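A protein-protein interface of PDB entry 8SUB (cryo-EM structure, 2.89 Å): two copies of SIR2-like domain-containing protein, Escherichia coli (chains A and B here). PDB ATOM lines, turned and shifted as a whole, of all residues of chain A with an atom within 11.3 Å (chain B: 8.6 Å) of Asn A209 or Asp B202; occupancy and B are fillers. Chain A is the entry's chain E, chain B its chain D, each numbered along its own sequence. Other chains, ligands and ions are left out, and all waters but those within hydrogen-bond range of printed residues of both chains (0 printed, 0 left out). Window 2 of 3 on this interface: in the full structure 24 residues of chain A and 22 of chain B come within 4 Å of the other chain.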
ATOM      1  N   GLN A 183      17.454  28.769 -25.799  1.00  0.00           N
ATOM      2  CA  GLN A 183      17.347  27.641 -26.717  1.00  0.00           C
ATOM      3  C   GLN A 183      18.120  27.937 -27.992  1.00  0.00           C
ATOM      4  O   GLN A 183      17.886  28.962 -28.637  1.00  0.00           O
ATOM      5  CB  GLN A 183      15.890  27.332 -27.053  1.00  0.00           C
ATOM      6  CG  GLN A 183      15.034  26.984 -25.857  1.00  0.00           C
ATOM      7  CD  GLN A 183      13.709  26.371 -26.257  1.00  0.00           C
ATOM      8  OE1 GLN A 183      13.514  25.988 -27.406  1.00  0.00           O
ATOM      9  NE2 GLN A 183      12.793  26.271 -25.307  1.00  0.00           N
ATOM     10  N   ALA A 204      11.300  29.935 -36.277  1.00  0.00           N
ATOM     11  CA  ALA A 204      11.398  30.930 -35.220  1.00  0.00           C
ATOM     12  C   ALA A 204      10.210  30.774 -34.283  1.00  0.00           C
ATOM     13  O   ALA A 204       9.220  30.118 -34.608  1.00  0.00           O
ATOM     14  CB  ALA A 204      11.454  32.347 -35.791  1.00  0.00           C
ATOM     15  N   PHE A 205      10.315  31.389 -33.110  1.00  0.00           N
ATOM     16  CA  PHE A 205       9.284  31.317 -32.084  1.00  0.00           C
ATOM     17  C   PHE A 205       8.456  32.597 -32.045  1.00  0.00           C
ATOM     18  O   PHE A 205       8.856  33.640 -32.564  1.00  0.00           O
ATOM     19  CB  PHE A 205       9.899  31.068 -30.704  1.00  0.00           C
ATOM     20  CG  PHE A 205      10.191  29.627 -30.417  1.00  0.00           C
ATOM     21  CD1 PHE A 205       9.341  28.633 -30.858  1.00  0.00           C
ATOM     22  CD2 PHE A 205      11.310  29.268 -29.690  1.00  0.00           C
ATOM     23  CE1 PHE A 205       9.607  27.311 -30.588  1.00  0.00           C
ATOM     24  CE2 PHE A 205      11.578  27.946 -29.418  1.00  0.00           C
ATOM     25  CZ  PHE A 205      10.728  26.967 -29.870  1.00  0.00           C
ATOM     26  N   ARG A 206       7.286  32.497 -31.418  1.00  0.00           N
ATOM     27  CA  ARG A 206       6.434  33.655 -31.172  1.00  0.00           C
ATOM     28  C   ARG A 206       5.520  33.341 -29.998  1.00  0.00           C
ATOM     29  O   ARG A 206       5.379  32.185 -29.593  1.00  0.00           O
ATOM     30  CB  ARG A 206       5.623  34.041 -32.412  1.00  0.00           C
ATOM     31  CG  ARG A 206       4.484  33.105 -32.722  1.00  0.00           C
ATOM     32  CD  ARG A 206       3.819  33.463 -34.037  1.00  0.00           C
ATOM     33  NE  ARG A 206       2.851  32.452 -34.439  1.00  0.00           N
ATOM     34  CZ  ARG A 206       1.600  32.400 -34.001  1.00  0.00           C
ATOM     35  NH1 ARG A 206       1.126  33.303 -33.160  1.00  0.00           N
ATOM     36  NH2 ARG A 206       0.808  31.418 -34.417  1.00  0.00           N
ATOM     37  N   ASN A 207       4.906  34.387 -29.451  1.00  0.00           N
ATOM     38  CA  ASN A 207       4.089  34.288 -28.248  1.00  0.00           C
ATOM     39  C   ASN A 207       2.614  34.410 -28.606  1.00  0.00           C
ATOM     40  O   ASN A 207       2.219  35.345 -29.310  1.00  0.00           O
ATOM     41  CB  ASN A 207       4.485  35.369 -27.243  1.00  0.00           C
ATOM     42  CG  ASN A 207       4.121  35.005 -25.820  1.00  0.00           C
ATOM     43  OD1 ASN A 207       3.086  34.392 -25.569  1.00  0.00           O
ATOM     44  ND2 ASN A 207       4.978  35.378 -24.879  1.00  0.00           N
ATOM     45  N   VAL A 208       1.802  33.474 -28.110  1.00  0.00           N
ATOM     46  CA  VAL A 208       0.390  33.426 -28.486  1.00  0.00           C
ATOM     47  C   VAL A 208      -0.455  34.476 -27.776  1.00  0.00           C
ATOM     48  O   VAL A 208      -1.537  34.817 -28.267  1.00  0.00           O
ATOM     49  CB  VAL A 208      -0.205  32.032 -28.220  1.00  0.00           C
ATOM     50  CG1 VAL A 208       0.508  30.982 -29.047  1.00  0.00           C
ATOM     51  CG2 VAL A 208      -0.127  31.693 -26.744  1.00  0.00           C
ATOM     52  N   ASN A 209      -0.004  35.001 -26.637  1.00  0.00           N
ATOM     53  CA  ASN A 209      -0.786  35.995 -25.911  1.00  0.00           C
ATOM     54  C   ASN A 209      -0.664  37.384 -26.528  1.00  0.00           C
ATOM     55  O   ASN A 209      -1.677  38.024 -26.824  1.00  0.00           O
ATOM     56  CB  ASN A 209      -0.359  36.039 -24.441  1.00  0.00           C
ATOM     57  CG  ASN A 209      -0.259  34.662 -23.820  1.00  0.00           C
ATOM     58  OD1 ASN A 209      -1.233  33.912 -23.782  1.00  0.00           O
ATOM     59  ND2 ASN A 209       0.925  34.323 -23.330  1.00  0.00           N
ATOM     60  N   ALA A 210       0.562  37.855 -26.734  1.00  0.00           N
ATOM     61  CA  ALA A 210       0.803  39.186 -27.282  1.00  0.00           C
ATOM     62  C   ALA A 210       0.215  39.347 -28.684  1.00  0.00           C
ATOM     63  O   ALA A 210      -0.123  38.367 -29.349  1.00  0.00           O
ATOM     64  CB  ALA A 210       2.296  39.482 -27.301  1.00  0.00           C
ATOM     65  N   GLY A 217      10.168  34.597 -24.798  1.00  0.00           N
ATOM     66  CA  GLY A 217       9.670  34.745 -26.153  1.00  0.00           C
ATOM     67  C   GLY A 217      10.775  34.791 -27.190  1.00  0.00           C
ATOM     68  O   GLY A 217      11.143  33.765 -27.762  1.00  0.00           O
ATOM     69  N   HIS A 218      11.315  35.990 -27.422  1.00  0.00           N
ATOM     70  CA  HIS A 218      12.389  36.201 -28.394  1.00  0.00           C
ATOM     71  C   HIS A 218      13.750  35.825 -27.804  1.00  0.00           C
ATOM     72  O   HIS A 218      14.690  36.615 -27.789  1.00  0.00           O
ATOM     73  CB  HIS A 218      12.404  37.650 -28.866  1.00  0.00           C
ATOM     74  CG  HIS A 218      11.251  38.027 -29.743  1.00  0.00           C
ATOM     75  ND1 HIS A 218      10.512  39.173 -29.543  1.00  0.00           N
ATOM     76  CD2 HIS A 218      10.722  37.423 -30.833  1.00  0.00           C
ATOM     77  CE1 HIS A 218       9.574  39.255 -30.469  1.00  0.00           C
ATOM     78  NE2 HIS A 218       9.678  38.203 -31.263  1.00  0.00           N
ATOM     79  N   TYR A 219      13.849  34.588 -27.315  1.00  0.00           N
ATOM     80  CA  TYR A 219      15.075  34.092 -26.687  1.00  0.00           C
ATOM     81  C   TYR A 219      15.514  32.818 -27.403  1.00  0.00           C
ATOM     82  O   TYR A 219      15.188  31.713 -26.966  1.00  0.00           O
ATOM     83  CB  TYR A 219      14.868  33.852 -25.192  1.00  0.00           C
ATOM     84  CG  TYR A 219      14.421  35.078 -24.424  1.00  0.00           C
ATOM     85  CD1 TYR A 219      14.889  36.341 -24.757  1.00  0.00           C
ATOM     86  CD2 TYR A 219      13.528  34.970 -23.366  1.00  0.00           C
ATOM     87  CE1 TYR A 219      14.479  37.463 -24.061  1.00  0.00           C
ATOM     88  CE2 TYR A 219      13.113  36.088 -22.662  1.00  0.00           C
ATOM     89  CZ  TYR A 219      13.591  37.331 -23.015  1.00  0.00           C
ATOM     90  OH  TYR A 219      13.183  38.443 -22.316  1.00  0.00           O
ATOM     91  N   PHE B 185       4.898  19.503 -28.219  1.00  0.00           N
ATOM     92  CA  PHE B 185       5.342  20.291 -27.078  1.00  0.00           C
ATOM     93  C   PHE B 185       4.792  19.662 -25.806  1.00  0.00           C
ATOM     94  O   PHE B 185       3.592  19.406 -25.717  1.00  0.00           O
ATOM     95  CB  PHE B 185       4.848  21.733 -27.200  1.00  0.00           C
ATOM     96  CG  PHE B 185       5.367  22.467 -28.410  1.00  0.00           C
ATOM     97  CD1 PHE B 185       6.700  22.820 -28.518  1.00  0.00           C
ATOM     98  CD2 PHE B 185       4.513  22.802 -29.443  1.00  0.00           C
ATOM     99  CE1 PHE B 185       7.162  23.494 -29.630  1.00  0.00           C
ATOM    100  CE2 PHE B 185       4.974  23.471 -30.553  1.00  0.00           C
ATOM    101  CZ  PHE B 185       6.297  23.818 -30.645  1.00  0.00           C
ATOM    102  N   GLY B 187       6.289  20.679 -22.411  1.00  0.00           N
ATOM    103  CA  GLY B 187       6.678  21.438 -21.242  1.00  0.00           C
ATOM    104  C   GLY B 187       8.144  21.370 -20.867  1.00  0.00           C
ATOM    105  O   GLY B 187       8.554  22.075 -19.944  1.00  0.00           O
ATOM    106  N   TYR B 197       9.490  23.559 -17.648  1.00  0.00           N
ATOM    107  CA  TYR B 197       9.158  24.976 -17.523  1.00  0.00           C
ATOM    108  C   TYR B 197       7.684  25.148 -17.864  1.00  0.00           C
ATOM    109  O   TYR B 197       7.290  24.901 -19.021  1.00  0.00           O
ATOM    110  CB  TYR B 197      10.009  25.844 -18.453  1.00  0.00           C
ATOM    111  CG  TYR B 197      11.487  25.885 -18.148  1.00  0.00           C
ATOM    112  CD1 TYR B 197      11.972  26.541 -17.028  1.00  0.00           C
ATOM    113  CD2 TYR B 197      12.400  25.276 -18.994  1.00  0.00           C
ATOM    114  CE1 TYR B 197      13.320  26.579 -16.757  1.00  0.00           C
ATOM    115  CE2 TYR B 197      13.746  25.308 -18.730  1.00  0.00           C
ATOM    116  CZ  TYR B 197      14.201  25.960 -17.613  1.00  0.00           C
ATOM    117  OH  TYR B 197      15.549  25.990 -17.358  1.00  0.00           O
ATOM    118  N   PRO B 198       6.839  25.578 -16.928  1.00  0.00           N
ATOM    119  CA  PRO B 198       5.423  25.793 -17.267  1.00  0.00           C
ATOM    120  C   PRO B 198       5.187  26.885 -18.300  1.00  0.00           C
ATOM    121  O   PRO B 198       4.115  26.908 -18.913  1.00  0.00           O
ATOM    122  CB  PRO B 198       4.788  26.152 -15.917  1.00  0.00           C
ATOM    123  CG  PRO B 198       5.910  26.611 -15.075  1.00  0.00           C
ATOM    124  CD  PRO B 198       7.110  25.835 -15.506  1.00  0.00           C
ATOM    125  N   GLN B 199       6.139  27.795 -18.511  1.00  0.00           N
ATOM    126  CA  GLN B 199       5.937  28.851 -19.496  1.00  0.00           C
ATOM    127  C   GLN B 199       6.013  28.335 -20.922  1.00  0.00           C
ATOM    128  O   GLN B 199       5.547  29.014 -21.840  1.00  0.00           O
ATOM    129  CB  GLN B 199       6.973  29.959 -19.319  1.00  0.00           C
ATOM    130  CG  GLN B 199       6.936  30.650 -17.978  1.00  0.00           C
ATOM    131  CD  GLN B 199       7.919  30.049 -17.004  1.00  0.00           C
ATOM    132  OE1 GLN B 199       9.030  29.679 -17.379  1.00  0.00           O
ATOM    133  NE2 GLN B 199       7.518  29.946 -15.743  1.00  0.00           N
ATOM    134  N   ASN B 200       6.581  27.163 -21.128  1.00  0.00           N
ATOM    135  CA  ASN B 200       6.771  26.615 -22.462  1.00  0.00           C
ATOM    136  C   ASN B 200       5.477  26.183 -23.120  1.00  0.00           C
ATOM    137  O   ASN B 200       5.558  25.513 -24.153  1.00  0.00           O
ATOM    138  CB  ASN B 200       7.735  25.431 -22.403  1.00  0.00           C
ATOM    139  CG  ASN B 200       9.182  25.857 -22.259  1.00  0.00           C
ATOM    140  OD1 ASN B 200       9.566  26.945 -22.679  1.00  0.00           O
ATOM    141  ND2 ASN B 200       9.994  24.993 -21.667  1.00  0.00           N
ATOM    142  N   PHE B 201       4.301  26.504 -22.581  1.00  0.00           N
ATOM    143  CA  PHE B 201       3.028  26.133 -23.184  1.00  0.00           C
ATOM    144  C   PHE B 201       2.394  27.276 -23.965  1.00  0.00           C
ATOM    145  O   PHE B 201       1.222  27.179 -24.339  1.00  0.00           O
ATOM    146  CB  PHE B 201       2.053  25.639 -22.109  1.00  0.00           C
ATOM    147  CG  PHE B 201       2.192  24.172 -21.784  1.00  0.00           C
ATOM    148  CD1 PHE B 201       2.066  23.213 -22.769  1.00  0.00           C
ATOM    149  CD2 PHE B 201       2.419  23.758 -20.488  1.00  0.00           C
ATOM    150  CE1 PHE B 201       2.182  21.876 -22.468  1.00  0.00           C
ATOM    151  CE2 PHE B 201       2.539  22.421 -20.188  1.00  0.00           C
ATOM    152  CZ  PHE B 201       2.418  21.481 -21.175  1.00  0.00           C
ATOM    153  N   ASP B 202       3.131  28.355 -24.219  1.00  0.00           N
ATOM    154  CA  ASP B 202       2.615  29.520 -24.931  1.00  0.00           C
ATOM    155  C   ASP B 202       3.502  29.883 -26.113  1.00  0.00           C
ATOM    156  O   ASP B 202       3.726  31.061 -26.399  1.00  0.00           O
ATOM    157  CB  ASP B 202       2.479  30.721 -23.999  1.00  0.00           C
ATOM    158  CG  ASP B 202       1.449  30.508 -22.913  1.00  0.00           C
ATOM    159  OD1 ASP B 202       0.304  30.146 -23.244  1.00  0.00           O
ATOM    160  OD2 ASP B 202       1.780  30.725 -21.728  1.00  0.00           O
ATOM    161  N   LEU B 203       4.016  28.885 -26.830  1.00  0.00           N
ATOM    162  CA  LEU B 203       4.912  29.120 -27.951  1.00  0.00           C
ATOM    163  C   LEU B 203       4.395  28.402 -29.189  1.00  0.00           C
ATOM    164  O   LEU B 203       3.749  27.357 -29.094  1.00  0.00           O
ATOM    165  CB  LEU B 203       6.332  28.648 -27.636  1.00  0.00           C
ATOM    166  CG  LEU B 203       7.015  29.302 -26.435  1.00  0.00           C
ATOM    167  CD1 LEU B 203       8.395  28.715 -26.224  1.00  0.00           C
ATOM    168  CD2 LEU B 203       7.092  30.806 -26.584  1.00  0.00           C
ATOM    169  N   ALA B 204       4.690  28.974 -30.356  1.00  0.00           N
ATOM    170  CA  ALA B 204       4.287  28.393 -31.628  1.00  0.00           C
ATOM    171  C   ALA B 204       5.336  28.723 -32.679  1.00  0.00           C
ATOM    172  O   ALA B 204       6.020  29.745 -32.593  1.00  0.00           O
ATOM    173  CB  ALA B 204       2.911  28.905 -32.064  1.00  0.00           C
ATOM    174  N   PHE B 205       5.452  27.855 -33.684  1.00  0.00           N
ATOM    175  CA  PHE B 205       6.444  28.087 -34.722  1.00  0.00           C
ATOM    176  C   PHE B 205       6.046  29.246 -35.630  1.00  0.00           C
ATOM    177  O   PHE B 205       4.932  29.772 -35.578  1.00  0.00           O
ATOM    178  CB  PHE B 205       6.684  26.850 -35.586  1.00  0.00           C
ATOM    179  CG  PHE B 205       7.372  25.727 -34.878  1.00  0.00           C
ATOM    180  CD1 PHE B 205       8.742  25.756 -34.691  1.00  0.00           C
ATOM    181  CD2 PHE B 205       6.677  24.604 -34.490  1.00  0.00           C
ATOM    182  CE1 PHE B 205       9.390  24.724 -34.064  1.00  0.00           C
ATOM    183  CE2 PHE B 205       7.327  23.561 -33.869  1.00  0.00           C
ATOM    184  CZ  PHE B 205       8.685  23.623 -33.660  1.00  0.00           C
ATOM    185  N   TYR B 222       0.193  19.799 -28.953  1.00  0.00           N
ATOM    186  CA  TYR B 222       0.488  19.796 -27.527  1.00  0.00           C
ATOM    187  C   TYR B 222       0.081  18.462 -26.923  1.00  0.00           C
ATOM    188  O   TYR B 222      -0.869  17.830 -27.380  1.00  0.00           O
ATOM    189  CB  TYR B 222      -0.240  20.938 -26.817  1.00  0.00           C
ATOM    190  CG  TYR B 222       0.204  22.307 -27.269  1.00  0.00           C
ATOM    191  CD1 TYR B 222       1.352  22.888 -26.756  1.00  0.00           C
ATOM    192  CD2 TYR B 222      -0.517  23.014 -28.216  1.00  0.00           C
ATOM    193  CE1 TYR B 222       1.770  24.130 -27.174  1.00  0.00           C
ATOM    194  CE2 TYR B 222      -0.106  24.261 -28.640  1.00  0.00           C
ATOM    195  CZ  TYR B 222       1.040  24.812 -28.114  1.00  0.00           C
ATOM    196  OH  TYR B 222       1.458  26.052 -28.530  1.00  0.00           O
ATOM    197  N   TYR B 224      -0.502  16.674 -23.035  1.00  0.00           N
ATOM    198  CA  TYR B 224      -0.603  16.792 -21.586  1.00  0.00           C
ATOM    199  C   TYR B 224      -0.761  15.403 -20.990  1.00  0.00           C
ATOM    200  O   TYR B 224      -1.740  14.714 -21.280  1.00  0.00           O
ATOM    201  CB  TYR B 224      -1.789  17.666 -21.185  1.00  0.00           C
ATOM    202  CG  TYR B 224      -1.848  19.020 -21.849  1.00  0.00           C
ATOM    203  CD1 TYR B 224      -2.341  19.165 -23.134  1.00  0.00           C
ATOM    204  CD2 TYR B 224      -1.443  20.155 -21.177  1.00  0.00           C
ATOM    205  CE1 TYR B 224      -2.408  20.399 -23.737  1.00  0.00           C
ATOM    206  CE2 TYR B 224      -1.502  21.390 -21.770  1.00  0.00           C
ATOM    207  CZ  TYR B 224      -1.988  21.508 -23.050  1.00  0.00           C
ATOM    208  OH  TYR B 224      -2.056  22.742 -23.648  1.00  0.00           O
ATOM    209  N   GLU B 286      -0.343  21.876 -12.389  1.00  0.00           N
ATOM    210  CA  GLU B 286      -0.209  22.560 -13.670  1.00  0.00           C
ATOM    211  C   GLU B 286      -0.993  21.850 -14.767  1.00  0.00           C
ATOM    212  O   GLU B 286      -1.705  22.497 -15.551  1.00  0.00           O
ATOM    213  CB  GLU B 286       1.267  22.663 -14.046  1.00  0.00           C
ATOM    214  CG  GLU B 286       1.541  23.409 -15.337  1.00  0.00           C
ATOM    215  CD  GLU B 286       1.197  24.880 -15.249  1.00  0.00           C
ATOM    216  OE1 GLU B 286       1.282  25.441 -14.140  1.00  0.00           O
ATOM    217  OE2 GLU B 286       0.848  25.477 -16.287  1.00  0.00           O
ATOM    218  N   ARG B 289      -4.706  22.316 -14.170  1.00  0.00           N
ATOM    219  CA  ARG B 289      -5.081  23.703 -14.376  1.00  0.00           C
ATOM    220  C   ARG B 289      -5.150  24.056 -15.847  1.00  0.00           C
ATOM    221  O   ARG B 289      -5.945  24.919 -16.227  1.00  0.00           O
ATOM    222  CB  ARG B 289      -4.084  24.624 -13.671  1.00  0.00           C
ATOM    223  CG  ARG B 289      -4.664  25.940 -13.186  1.00  0.00           C
ATOM    224  CD  ARG B 289      -4.244  27.097 -14.071  1.00  0.00           C
ATOM    225  NE  ARG B 289      -2.795  27.234 -14.131  1.00  0.00           N
ATOM    226  CZ  ARG B 289      -2.151  27.924 -15.062  1.00  0.00           C
ATOM    227  NH1 ARG B 289      -2.799  28.577 -16.011  1.00  0.00           N
ATOM    228  NH2 ARG B 289      -0.823  27.955 -15.042  1.00  0.00           N
ATOM    229  N   ARG B 290      -4.321  23.426 -16.676  1.00  0.00           N
ATOM    230  CA  ARG B 290      -4.450  23.597 -18.117  1.00  0.00           C
ATOM    231  C   ARG B 290      -5.615  22.811 -18.703  1.00  0.00           C
ATOM    232  O   ARG B 290      -6.190  23.240 -19.708  1.00  0.00           O
ATOM    233  CB  ARG B 290      -3.151  23.197 -18.816  1.00  0.00           C
ATOM    234  CG  ARG B 290      -1.951  24.048 -18.442  1.00  0.00           C
ATOM    235  CD  ARG B 290      -1.709  25.151 -19.448  1.00  0.00           C
ATOM    236  NE  ARG B 290      -0.603  26.013 -19.051  1.00  0.00           N
ATOM    237  CZ  ARG B 290      -0.377  27.225 -19.542  1.00  0.00           C
ATOM    238  NH1 ARG B 290      -1.173  27.761 -20.451  1.00  0.00           N
ATOM    239  NH2 ARG B 290       0.670  27.915 -19.107  1.00  0.00           N
ATOM    240  N   GLU B 293      -8.946  24.851 -18.067  1.00  0.00           N
ATOM    241  CA  GLU B 293      -9.006  26.098 -18.820  1.00  0.00           C
ATOM    242  C   GLU B 293      -9.409  25.853 -20.270  1.00  0.00           C
ATOM    243  O   GLU B 293      -9.921  26.756 -20.939  1.00  0.00           O
ATOM    244  CB  GLU B 293      -7.654  26.801 -18.737  1.00  0.00           C
ATOM    245  CG  GLU B 293      -7.507  28.040 -19.586  1.00  0.00           C
ATOM    246  CD  GLU B 293      -6.134  28.654 -19.457  1.00  0.00           C
ATOM    247  OE1 GLU B 293      -5.325  28.136 -18.661  1.00  0.00           O
ATOM    248  OE2 GLU B 293      -5.861  29.653 -20.154  1.00  0.00           O
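Ala B204 touches its own counterpart, Ala A204.
Ala A204 touches Phe B205, and with the chains exchanged Phe A205 touches Ala B204.
OD1 of Asp B202 lies within salt-bridge range of NH1 of Arg B290 (3.96 Å).
The side-chain hydroxyl (OH) of Tyr B222 is in hydrogen-bond range of the backbone carbonyl oxygen (O) of Leu B203 (2.7 Å).
The side-chain amide nitrogen (ND2) of Asn A209 lies within hydrogen-bond range of the side-chain amide oxygen (OD1) of Asn A207 (3.1 Å).
Asn A209 touches just one residue of chain B: Asp B202.
Of chain A, only Arg A206, Asn A207, Val A208 and Asn A209 come within 4 Å of Asp B202.
Val A208 touches just one residue of chain B: Asp B202.
Leu B203 touches just one residue of chain A: Arg A206.
Printed residues of chain A within 4 Å of Ala B204: Ala A204 (3.8 Å), Phe A205 (3.7 Å) and Arg A206 (3.2 Å).
Of the printed residues of chain B, Ala A204 touches Ala B204 (3.8 Å) and Phe B205 (3.4 Å).
Printed residues of chain B within 4 Å of Arg A206: Asp B202 (3.8 Å), Leu B203 (3.5 Å), Ala B204 (3.2 Å) and Phe B205 (3.6 Å).
Printed residues of chain B within 4 Å of Asn A207: Asp B202.
Gln B199 touches none of the printed residues of chain A.
The nearest residue of chain B that does not touch Asn A209 is Arg B290 (7.0 Å).
The nearest residue of chain A that does not touch Asp B202 is Gly A217 (7.0 Å).
Of the 11 printed residues of chain A, 6 touch a printed residue of chain B.
Hydrophobic or aromatic side chains of chain A that line the printed part of chain B: Phe A205 and Val A208.
Hydrophobic or aromatic side chains of chain B that line the printed part of chain A: Leu B203.
Along chain B the printed residues that touch a printed residue of chain A span positions 202 to 205.
Among the printed residues, no Asp or Glu carboxylate lies within 4 Å of a Lys or Arg side-chain nitrogen of the other chain.
O of Ala A204 touches O of Ala B204 (3.8 Å).
O of Ala A204 touches CA of Phe B205 (3.4 Å).
Phe A205 touches Ala B204.
Arg A206 touches Asp B202 (O to O, 3.8 Å).
CA of Leu B203 touches O of Arg A206, 3.5 Å away.
Arg A206 touches Phe B205 (NE to O, 3.6 Å).
O of Asp B202 touches N of Val A208, 3.5 Å away.
Asn A209 touches Asp B202 (ND2 to CG, 3.9 Å).
The backbone carbonyl oxygen (O) of Asp B202 sits close to the side-chain amide oxygen (OD1) of Asn A207 (3.5 Å).
N of Arg A206 sits at hydrogen-bond distance from O of Ala B204, 3.2 Å away.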
